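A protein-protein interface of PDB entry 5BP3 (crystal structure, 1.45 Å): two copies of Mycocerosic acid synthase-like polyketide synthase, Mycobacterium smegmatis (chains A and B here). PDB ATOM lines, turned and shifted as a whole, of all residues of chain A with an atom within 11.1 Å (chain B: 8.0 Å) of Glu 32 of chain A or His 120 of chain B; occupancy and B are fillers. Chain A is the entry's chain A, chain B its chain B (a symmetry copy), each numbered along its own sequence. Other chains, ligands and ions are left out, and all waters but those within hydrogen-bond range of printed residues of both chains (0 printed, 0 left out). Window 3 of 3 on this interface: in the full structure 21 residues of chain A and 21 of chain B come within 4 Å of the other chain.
The backbone carbonyl oxygen of Pro 30 of chain A is in hydrogen-bond range of the guanidinium group of Arg 125 of chain B (2.5 Å). NE1 of Trp 102 of chain B lies within hydrogen-bond range of O of Val 28 of chain A, 2.7 Å away.
The backbone carbonyl oxygen of Trp 102 of chain B sits at hydrogen-bond distance from the backbone NH of Glu 118 of chain B (2.9 Å). OE1 of Glu 118 of chain B lies within salt-bridge range of NH2 of Arg 125 of chain B (2.9 Å). The side-chain amide nitrogen (NE2) of Gln 31 of chain A lies within hydrogen-bond range of the side-chain carboxylate (OE1) of Glu 35 of chain A (3.5 Å).
Among the printed residues, pairs that only touch across the chains: Pro 30 of chain A with Trp 102 of chain B (3.7 Å), Pro 30 of chain A with Glu 118 of chain B (3.5 Å), Gln 31 of chain A with His 120 of chain B (3.9 Å) and Glu 32 of chain A with His 120 of chain B (3.7 Å).
Printed residues of chain B within 4 Å of Glu 32 of chain A: His 120 (3.7 Å). Of the printed residues of chain A, His 120 of chain B touches Gln 31 (3.9 Å) and Glu 32 (3.7 Å). Glu 118 of chain B touches one residue of chain A. No residue of chain A comes within 4 Å of Thr 119 of chain B. Of the printed residues of chain B, Gln 31 of chain A touches His 120 (3.9 Å). Printed residues of chain B within 4 Å of Val 28 of chain A: Trp 102 (2.7 Å). Of the printed residues of chain A, Arg 125 of chain B touches Pro 30. Thr 99 of chain B touches none of the printed residues of chain A. Gln 127 of chain B touches none of the printed residues of chain A. The nearest printed residue of chain B that does not touch Glu 32 of chain A is Arg 125 of chain B (6.6 Å). The nearest printed residue of chain A that does not touch Arg 125 of chain B is Gln 31 of chain A (4.6 Å).
Of the 15 printed residues of chain A, 4 touch a printed residue of chain B. Printed residues of chain A that touch a printed residue of chain B: Val 28, Pro 30, Gln 31 and Glu 32. Of the 12 printed residues of chain B, 4 touch a printed residue of chain A. Printed residues of chain B that touch a printed residue of chain A: Trp 102, Glu 118, His 120 and Arg 125. Hydrophobic or aromatic side chains of chain B that line the printed part of chain A: Trp 102 and His 120.
No position is printed for both chains. Of the 6 pairs that touch across the chains among the printed residues, none has its exchanged pair printed and touching as well.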
ATOM      1  N   VAL A  28      -4.588   5.277  -1.837  1.00  0.00           N
ATOM      2  CA  VAL A  28      -4.168   5.362  -3.218  1.00  0.00           C
ATOM      3  C   VAL A  28      -5.252   4.685  -4.046  1.00  0.00           C
ATOM      4  O   VAL A  28      -5.733   3.617  -3.659  1.00  0.00           O
ATOM      5  CB  VAL A  28      -2.827   4.682  -3.385  1.00  0.00           C
ATOM      6  CG1 VAL A  28      -2.450   4.599  -4.835  1.00  0.00           C
ATOM      7  CG2 VAL A  28      -1.770   5.426  -2.591  1.00  0.00           C
ATOM      8  N   LEU A  29      -5.676   5.267  -5.150  1.00  0.00           N
ATOM      9  CA  LEU A  29      -6.739   4.685  -5.953  1.00  0.00           C
ATOM     10  C   LEU A  29      -6.207   3.456  -6.687  1.00  0.00           C
ATOM     11  O   LEU A  29      -5.021   3.395  -7.019  1.00  0.00           O
ATOM     12  CB  LEU A  29      -7.290   5.699  -6.956  1.00  0.00           C
ATOM     13  CG  LEU A  29      -7.860   6.993  -6.366  1.00  0.00           C
ATOM     14  CD1 LEU A  29      -8.453   7.847  -7.487  1.00  0.00           C
ATOM     15  CD2 LEU A  29      -8.897   6.711  -5.294  1.00  0.00           C
ATOM     16  N   PRO A  30      -7.080   2.461  -6.925  1.00  0.00           N
ATOM     17  CA  PRO A  30      -6.674   1.247  -7.636  1.00  0.00           C
ATOM     18  C   PRO A  30      -6.670   1.465  -9.140  1.00  0.00           C
ATOM     19  O   PRO A  30      -7.486   0.886  -9.857  1.00  0.00           O
ATOM     20  CB  PRO A  30      -7.764   0.249  -7.247  1.00  0.00           C
ATOM     21  CG  PRO A  30      -8.987   1.092  -7.141  1.00  0.00           C
ATOM     22  CD  PRO A  30      -8.510   2.439  -6.581  1.00  0.00           C
ATOM     23  N   GLN A  31      -5.757   2.308  -9.615  1.00  0.00           N
ATOM     24  CA  GLN A  31      -5.698   2.619 -11.034  1.00  0.00           C
ATOM     25  C   GLN A  31      -4.349   3.221 -11.412  1.00  0.00           C
ATOM     26  O   GLN A  31      -3.497   3.468 -10.551  1.00  0.00           O
ATOM     27  CB  GLN A  31      -6.817   3.599 -11.400  1.00  0.00           C
ATOM     28  CG  GLN A  31      -6.674   4.958 -10.708  1.00  0.00           C
ATOM     29  CD  GLN A  31      -7.885   5.857 -10.896  1.00  0.00           C
ATOM     30  OE1 GLN A  31      -9.023   5.444 -10.654  1.00  0.00           O
ATOM     31  NE2 GLN A  31      -7.646   7.089 -11.330  1.00  0.00           N
ATOM     32  N   GLU A  32      -4.178   3.459 -12.707  1.00  0.00           N
ATOM     33  CA  GLU A  32      -3.017   4.160 -13.231  1.00  0.00           C
ATOM     34  C   GLU A  32      -3.530   5.386 -13.959  1.00  0.00           C
ATOM     35  O   GLU A  32      -4.607   5.337 -14.557  1.00  0.00           O
ATOM     36  CB  GLU A  32      -2.248   3.274 -14.209  1.00  0.00           C
ATOM     37  CG  GLU A  32      -1.530   2.099 -13.562  1.00  0.00           C
ATOM     38  CD  GLU A  32      -0.365   2.538 -12.687  1.00  0.00           C
ATOM     39  OE1 GLU A  32       0.032   3.728 -12.757  1.00  0.00           O
ATOM     40  OE2 GLU A  32       0.156   1.695 -11.927  1.00  0.00           O
ATOM     41  N   PRO A  33      -2.778   6.493 -13.912  1.00  0.00           N
ATOM     42  CA  PRO A  33      -1.522   6.706 -13.184  1.00  0.00           C
ATOM     43  C   PRO A  33      -1.752   6.783 -11.683  1.00  0.00           C
ATOM     44  O   PRO A  33      -2.899   6.759 -11.234  1.00  0.00           O
ATOM     45  CB  PRO A  33      -1.035   8.070 -13.692  1.00  0.00           C
ATOM     46  CG  PRO A  33      -1.864   8.382 -14.894  1.00  0.00           C
ATOM     47  CD  PRO A  33      -3.168   7.687 -14.673  1.00  0.00           C
ATOM     48  N   GLU A  34      -0.665   6.884 -10.925  1.00  0.00           N
ATOM     49  CA  GLU A  34      -0.747   6.934  -9.479  1.00  0.00           C
ATOM     50  C   GLU A  34      -1.561   8.140  -9.026  1.00  0.00           C
ATOM     51  O   GLU A  34      -1.247   9.290  -9.359  1.00  0.00           O
ATOM     52  CB  GLU A  34       0.659   7.006  -8.884  1.00  0.00           C
ATOM     53  CG  GLU A  34       0.699   7.193  -7.382  1.00  0.00           C
ATOM     54  CD  GLU A  34       2.104   7.403  -6.853  1.00  0.00           C
ATOM     55  OE1 GLU A  34       3.058   7.361  -7.666  1.00  0.00           O
ATOM     56  OE2 GLU A  34       2.256   7.615  -5.625  1.00  0.00           O
ATOM     57  N   GLU A  35      -2.599   7.869  -8.243  1.00  0.00           N
ATOM     58  CA  GLU A  35      -3.440   8.917  -7.694  1.00  0.00           C
ATOM     59  C   GLU A  35      -3.827   8.680  -6.243  1.00  0.00           C
ATOM     60  O   GLU A  35      -4.216   7.587  -5.857  1.00  0.00           O
ATOM     61  CB  GLU A  35      -4.674   9.123  -8.562  1.00  0.00           C
ATOM     62  CG  GLU A  35      -5.552  10.277  -8.095  1.00  0.00           C
ATOM     63  CD  GLU A  35      -6.606  10.664  -9.106  1.00  0.00           C
ATOM     64  OE1 GLU A  35      -6.526  10.210 -10.270  1.00  0.00           O
ATOM     65  OE2 GLU A  35      -7.519  11.429  -8.728  1.00  0.00           O
ATOM     66  N   HIS A  36      -3.739   9.728  -5.447  1.00  0.00           N
ATOM     67  CA  HIS A  36      -4.003   9.713  -4.029  1.00  0.00           C
ATOM     68  C   HIS A  36      -5.309  10.447  -3.725  1.00  0.00           C
ATOM     69  O   HIS A  36      -5.647  11.439  -4.372  1.00  0.00           O
ATOM     70  CB  HIS A  36      -2.858  10.409  -3.267  1.00  0.00           C
ATOM     71  CG  HIS A  36      -1.537   9.723  -3.412  1.00  0.00           C
ATOM     72  ND1 HIS A  36      -0.903   9.104  -2.357  1.00  0.00           N
ATOM     73  CD2 HIS A  36      -0.733   9.552  -4.489  1.00  0.00           C
ATOM     74  CE1 HIS A  36       0.227   8.561  -2.782  1.00  0.00           C
ATOM     75  NE2 HIS A  36       0.357   8.824  -4.070  1.00  0.00           N
ATOM     76  N   ALA A 105      -4.264  14.043  -5.378  1.00  0.00           N
ATOM     77  CA  ALA A 105      -2.962  14.289  -5.950  1.00  0.00           C
ATOM     78  C   ALA A 105      -2.716  13.249  -7.014  1.00  0.00           C
ATOM     79  O   ALA A 105      -2.746  12.059  -6.733  1.00  0.00           O
ATOM     80  CB  ALA A 105      -1.893  14.270  -4.900  1.00  0.00           C
ATOM     81  N   ALA A 106      -2.502  13.682  -8.243  1.00  0.00           N
ATOM     82  CA  ALA A 106      -2.318  12.773  -9.369  1.00  0.00           C
ATOM     83  C   ALA A 106      -0.944  13.002  -9.943  1.00  0.00           C
ATOM     84  O   ALA A 106      -0.609  14.126 -10.347  1.00  0.00           O
ATOM     85  CB  ALA A 106      -3.360  13.026 -10.416  1.00  0.00           C
ATOM     86  N   VAL A 107      -0.137  11.954  -9.965  1.00  0.00           N
ATOM     87  CA  VAL A 107       1.210  12.036 -10.490  1.00  0.00           C
ATOM     88  C   VAL A 107       1.164  12.097 -12.011  1.00  0.00           C
ATOM     89  O   VAL A 107       0.623  11.201 -12.662  1.00  0.00           O
ATOM     90  CB  VAL A 107       2.040  10.834 -10.039  1.00  0.00           C
ATOM     91  CG1 VAL A 107       3.443  10.916 -10.630  1.00  0.00           C
ATOM     92  CG2 VAL A 107       2.083  10.790  -8.524  1.00  0.00           C
ATOM     93  N   THR A 108       1.726  13.165 -12.581  1.00  0.00           N
ATOM     94  CA  THR A 108       1.713  13.334 -14.034  1.00  0.00           C
ATOM     95  C   THR A 108       3.046  12.989 -14.678  1.00  0.00           C
ATOM     96  O   THR A 108       3.123  12.736 -15.880  1.00  0.00           O
ATOM     97  CB  THR A 108       1.413  14.771 -14.426  1.00  0.00           C
ATOM     98  OG1 THR A 108       2.338  15.633 -13.756  1.00  0.00           O
ATOM     99  CG2 THR A 108      -0.014  15.137 -14.055  1.00  0.00           C
ATOM    100  N   ALA A 109       4.104  13.009 -13.885  1.00  0.00           N
ATOM    101  CA  ALA A 109       5.414  12.625 -14.376  1.00  0.00           C
ATOM    102  C   ALA A 109       6.237  12.457 -13.135  1.00  0.00           C
ATOM    103  O   ALA A 109       5.826  12.906 -12.075  1.00  0.00           O
ATOM    104  CB  ALA A 109       6.003  13.704 -15.259  1.00  0.00           C
ATOM    105  N   PRO A 110       7.389  11.798 -13.252  1.00  0.00           N
ATOM    106  CA  PRO A 110       8.232  11.657 -12.068  1.00  0.00           C
ATOM    107  C   PRO A 110       8.506  13.019 -11.456  1.00  0.00           C
ATOM    108  O   PRO A 110       8.849  13.975 -12.163  1.00  0.00           O
ATOM    109  CB  PRO A 110       9.510  11.027 -12.620  1.00  0.00           C
ATOM    110  CG  PRO A 110       9.057  10.263 -13.836  1.00  0.00           C
ATOM    111  CD  PRO A 110       7.948  11.102 -14.425  1.00  0.00           C
ATOM    112  N   LEU B  93      -6.185 -15.695  -4.256  1.00  0.00           N
ATOM    113  CA  LEU B  93      -5.215 -14.613  -4.127  1.00  0.00           C
ATOM    114  C   LEU B  93      -3.965 -15.123  -3.439  1.00  0.00           C
ATOM    115  O   LEU B  93      -3.988 -15.471  -2.242  1.00  0.00           O
ATOM    116  CB  LEU B  93      -5.825 -13.493  -3.302  1.00  0.00           C
ATOM    117  CG  LEU B  93      -4.889 -12.319  -2.971  1.00  0.00           C
ATOM    118  CD1 LEU B  93      -4.285 -11.654  -4.225  1.00  0.00           C
ATOM    119  CD2 LEU B  93      -5.657 -11.298  -2.169  1.00  0.00           C
ATOM    120  N   THR B  99       0.547  -7.284   0.196  1.00  0.00           N
ATOM    121  CA  THR B  99      -0.486  -7.554  -0.792  1.00  0.00           C
ATOM    122  C   THR B  99      -1.617  -6.539  -0.679  1.00  0.00           C
ATOM    123  O   THR B  99      -2.557  -6.696   0.063  1.00  0.00           O
ATOM    124  CB  THR B  99      -1.034  -8.995  -0.626  1.00  0.00           C
ATOM    125  OG1 THR B  99       0.041  -9.927  -0.774  1.00  0.00           O
ATOM    126  CG2 THR B  99      -2.103  -9.252  -1.672  1.00  0.00           C
ATOM    127  N   PRO B 100      -1.498  -5.415  -1.398  1.00  0.00           N
ATOM    128  CA  PRO B 100      -2.578  -4.435  -1.305  1.00  0.00           C
ATOM    129  C   PRO B 100      -3.916  -4.943  -1.825  1.00  0.00           C
ATOM    130  O   PRO B 100      -3.965  -5.655  -2.834  1.00  0.00           O
ATOM    131  CB  PRO B 100      -2.066  -3.264  -2.184  1.00  0.00           C
ATOM    132  CG  PRO B 100      -0.634  -3.509  -2.332  1.00  0.00           C
ATOM    133  CD  PRO B 100      -0.418  -4.976  -2.284  1.00  0.00           C
ATOM    134  N   VAL B 101      -4.990  -4.584  -1.126  1.00  0.00           N
ATOM    135  CA  VAL B 101      -6.337  -4.898  -1.562  1.00  0.00           C
ATOM    136  C   VAL B 101      -7.198  -3.663  -1.434  1.00  0.00           C
ATOM    137  O   VAL B 101      -7.019  -2.847  -0.512  1.00  0.00           O
ATOM    138  CB  VAL B 101      -6.987  -6.042  -0.727  1.00  0.00           C
ATOM    139  CG1 VAL B 101      -6.433  -7.396  -1.134  1.00  0.00           C
ATOM    140  CG2 VAL B 101      -6.815  -5.782   0.782  1.00  0.00           C
ATOM    141  N   TRP B 102      -8.104  -3.518  -2.387  1.00  0.00           N
ATOM    142  CA  TRP B 102      -9.058  -2.440  -2.373  1.00  0.00           C
ATOM    143  C   TRP B 102     -10.463  -3.015  -2.277  1.00  0.00           C
ATOM    144  O   TRP B 102     -10.850  -3.952  -3.020  1.00  0.00           O
ATOM    145  CB  TRP B 102      -8.918  -1.583  -3.623  1.00  0.00           C
ATOM    146  CG  TRP B 102      -7.658  -0.775  -3.680  1.00  0.00           C
ATOM    147  CD1 TRP B 102      -7.519   0.539  -3.324  1.00  0.00           C
ATOM    148  CD2 TRP B 102      -6.375  -1.209  -4.126  1.00  0.00           C
ATOM    149  NE1 TRP B 102      -6.229   0.936  -3.513  1.00  0.00           N
ATOM    150  CE2 TRP B 102      -5.500  -0.096  -4.027  1.00  0.00           C
ATOM    151  CE3 TRP B 102      -5.874  -2.413  -4.623  1.00  0.00           C
ATOM    152  CZ2 TRP B 102      -4.156  -0.178  -4.367  1.00  0.00           C
ATOM    153  CZ3 TRP B 102      -4.548  -2.491  -4.967  1.00  0.00           C
ATOM    154  CH2 TRP B 102      -3.697  -1.379  -4.852  1.00  0.00           C
ATOM    155  N   GLU B 118     -10.792  -6.136  -4.879  1.00  0.00           N
ATOM    156  CA  GLU B 118      -9.915  -6.255  -6.037  1.00  0.00           C
ATOM    157  C   GLU B 118      -8.467  -6.012  -5.670  1.00  0.00           C
ATOM    158  O   GLU B 118      -8.158  -5.397  -4.635  1.00  0.00           O
ATOM    159  CB  GLU B 118     -10.363  -5.338  -7.187  1.00  0.00           C
ATOM    160  CG  GLU B 118     -10.278  -3.881  -6.864  1.00  0.00           C
ATOM    161  CD  GLU B 118     -10.894  -2.987  -7.954  1.00  0.00           C
ATOM    162  OE1 GLU B 118     -10.841  -1.769  -7.805  1.00  0.00           O
ATOM    163  OE2 GLU B 118     -11.453  -3.506  -8.949  1.00  0.00           O
ATOM    164  N   THR B 119      -7.592  -6.604  -6.481  1.00  0.00           N
ATOM    165  CA  THR B 119      -6.161  -6.334  -6.400  1.00  0.00           C
ATOM    166  C   THR B 119      -5.736  -5.720  -7.714  1.00  0.00           C
ATOM    167  O   THR B 119      -6.447  -5.850  -8.711  1.00  0.00           O
ATOM    168  CB  THR B 119      -5.363  -7.612  -6.126  1.00  0.00           C
ATOM    169  OG1 THR B 119      -5.734  -8.618  -7.065  1.00  0.00           O
ATOM    170  CG2 THR B 119      -5.667  -8.126  -4.746  1.00  0.00           C
ATOM    171  N   HIS B 120      -4.597  -5.032  -7.699  1.00  0.00           N
ATOM    172  CA  HIS B 120      -4.135  -4.233  -8.831  1.00  0.00           C
ATOM    173  C   HIS B 120      -2.621  -4.236  -8.915  1.00  0.00           C
ATOM    174  O   HIS B 120      -2.066  -4.383  -9.998  1.00  0.00           O
ATOM    175  CB  HIS B 120      -4.632  -2.792  -8.720  1.00  0.00           C
ATOM    176  CG  HIS B 120      -4.009  -1.863  -9.716  1.00  0.00           C
ATOM    177  ND1 HIS B 120      -2.980  -1.004  -9.392  1.00  0.00           N
ATOM    178  CD2 HIS B 120      -4.255  -1.673 -11.034  1.00  0.00           C
ATOM    179  CE1 HIS B 120      -2.627  -0.318 -10.465  1.00  0.00           C
ATOM    180  NE2 HIS B 120      -3.385  -0.705 -11.475  1.00  0.00           N
ATOM    181  N   ARG B 125      -5.843  -5.192 -13.038  1.00  0.00           N
ATOM    182  CA  ARG B 125      -6.771  -5.352 -11.913  1.00  0.00           C
ATOM    183  C   ARG B 125      -7.589  -6.648 -11.977  1.00  0.00           C
ATOM    184  O   ARG B 125      -8.154  -6.992 -13.022  1.00  0.00           O
ATOM    185  CB  ARG B 125      -7.706  -4.146 -11.809  1.00  0.00           C
ATOM    186  CG  ARG B 125      -8.563  -3.918 -13.045  1.00  0.00           C
ATOM    187  CD  ARG B 125      -8.778  -2.426 -13.319  1.00  0.00           C
ATOM    188  NE  ARG B 125      -9.741  -1.812 -12.407  1.00  0.00           N
ATOM    189  CZ  ARG B 125      -9.429  -1.315 -11.217  1.00  0.00           C
ATOM    190  NH1 ARG B 125      -8.178  -1.372 -10.787  1.00  0.00           N
ATOM    191  NH2 ARG B 125     -10.367  -0.769 -10.454  1.00  0.00           N
ATOM    192  N   THR B 126      -7.660  -7.340 -10.843  1.00  0.00           N
ATOM    193  CA  THR B 126      -8.331  -8.632 -10.743  1.00  0.00           C
ATOM    194  C   THR B 126      -9.358  -8.599  -9.620  1.00  0.00           C
ATOM    195  O   THR B 126      -9.024  -8.292  -8.465  1.00  0.00           O
ATOM    196  CB  THR B 126      -7.309  -9.727 -10.433  1.00  0.00           C
ATOM    197  OG1 THR B 126      -6.312  -9.746 -11.454  1.00  0.00           O
ATOM    198  CG2 THR B 126      -7.961 -11.096 -10.361  1.00  0.00           C
ATOM    199  N   GLN B 127     -10.597  -8.948  -9.961  1.00  0.00           N
ATOM    200  CA  GLN B 127     -11.670  -9.074  -8.983  1.00  0.00           C
ATOM    201  C   GLN B 127     -11.447 -10.322  -8.133  1.00  0.00           C
ATOM    202  O   GLN B 127     -11.162 -11.405  -8.663  1.00  0.00           O
ATOM    203  CB  GLN B 127     -13.007  -9.188  -9.711  1.00  0.00           C
ATOM    204  CG  GLN B 127     -14.240  -8.931  -8.856  1.00  0.00           C
ATOM    205  CD  GLN B 127     -14.395  -7.470  -8.444  1.00  0.00           C
ATOM    206  OE1 GLN B 127     -13.829  -6.568  -9.056  1.00  0.00           O
ATOM    207  NE2 GLN B 127     -15.167  -7.240  -7.394  1.00  0.00           N
ATOM    208  N   ARG B 128     -11.569 -10.164  -6.826  1.00  0.00           N
ATOM    209  CA  ARG B 128     -11.296 -11.243  -5.893  1.00  0.00           C
ATOM    210  C   ARG B 128     -12.554 -11.703  -5.195  1.00  0.00           C
ATOM    211  O   ARG B 128     -12.670 -12.866  -4.876  1.00  0.00           O
ATOM    212  CB  ARG B 128     -10.266 -10.819  -4.847  1.00  0.00           C
ATOM    213  CG  ARG B 128      -8.909 -10.480  -5.415  1.00  0.00           C
ATOM    214  CD  ARG B 128      -8.301 -11.642  -6.177  1.00  0.00           C
ATOM    215  NE  ARG B 128      -7.018 -11.283  -6.757  1.00  0.00           N
ATOM    216  CZ  ARG B 128      -6.181 -12.141  -7.328  1.00  0.00           C
ATOM    217  NH1 ARG B 128      -5.024 -11.703  -7.817  1.00  0.00           N
ATOM    218  NH2 ARG B 128      -6.488 -13.431  -7.401  1.00  0.00           N
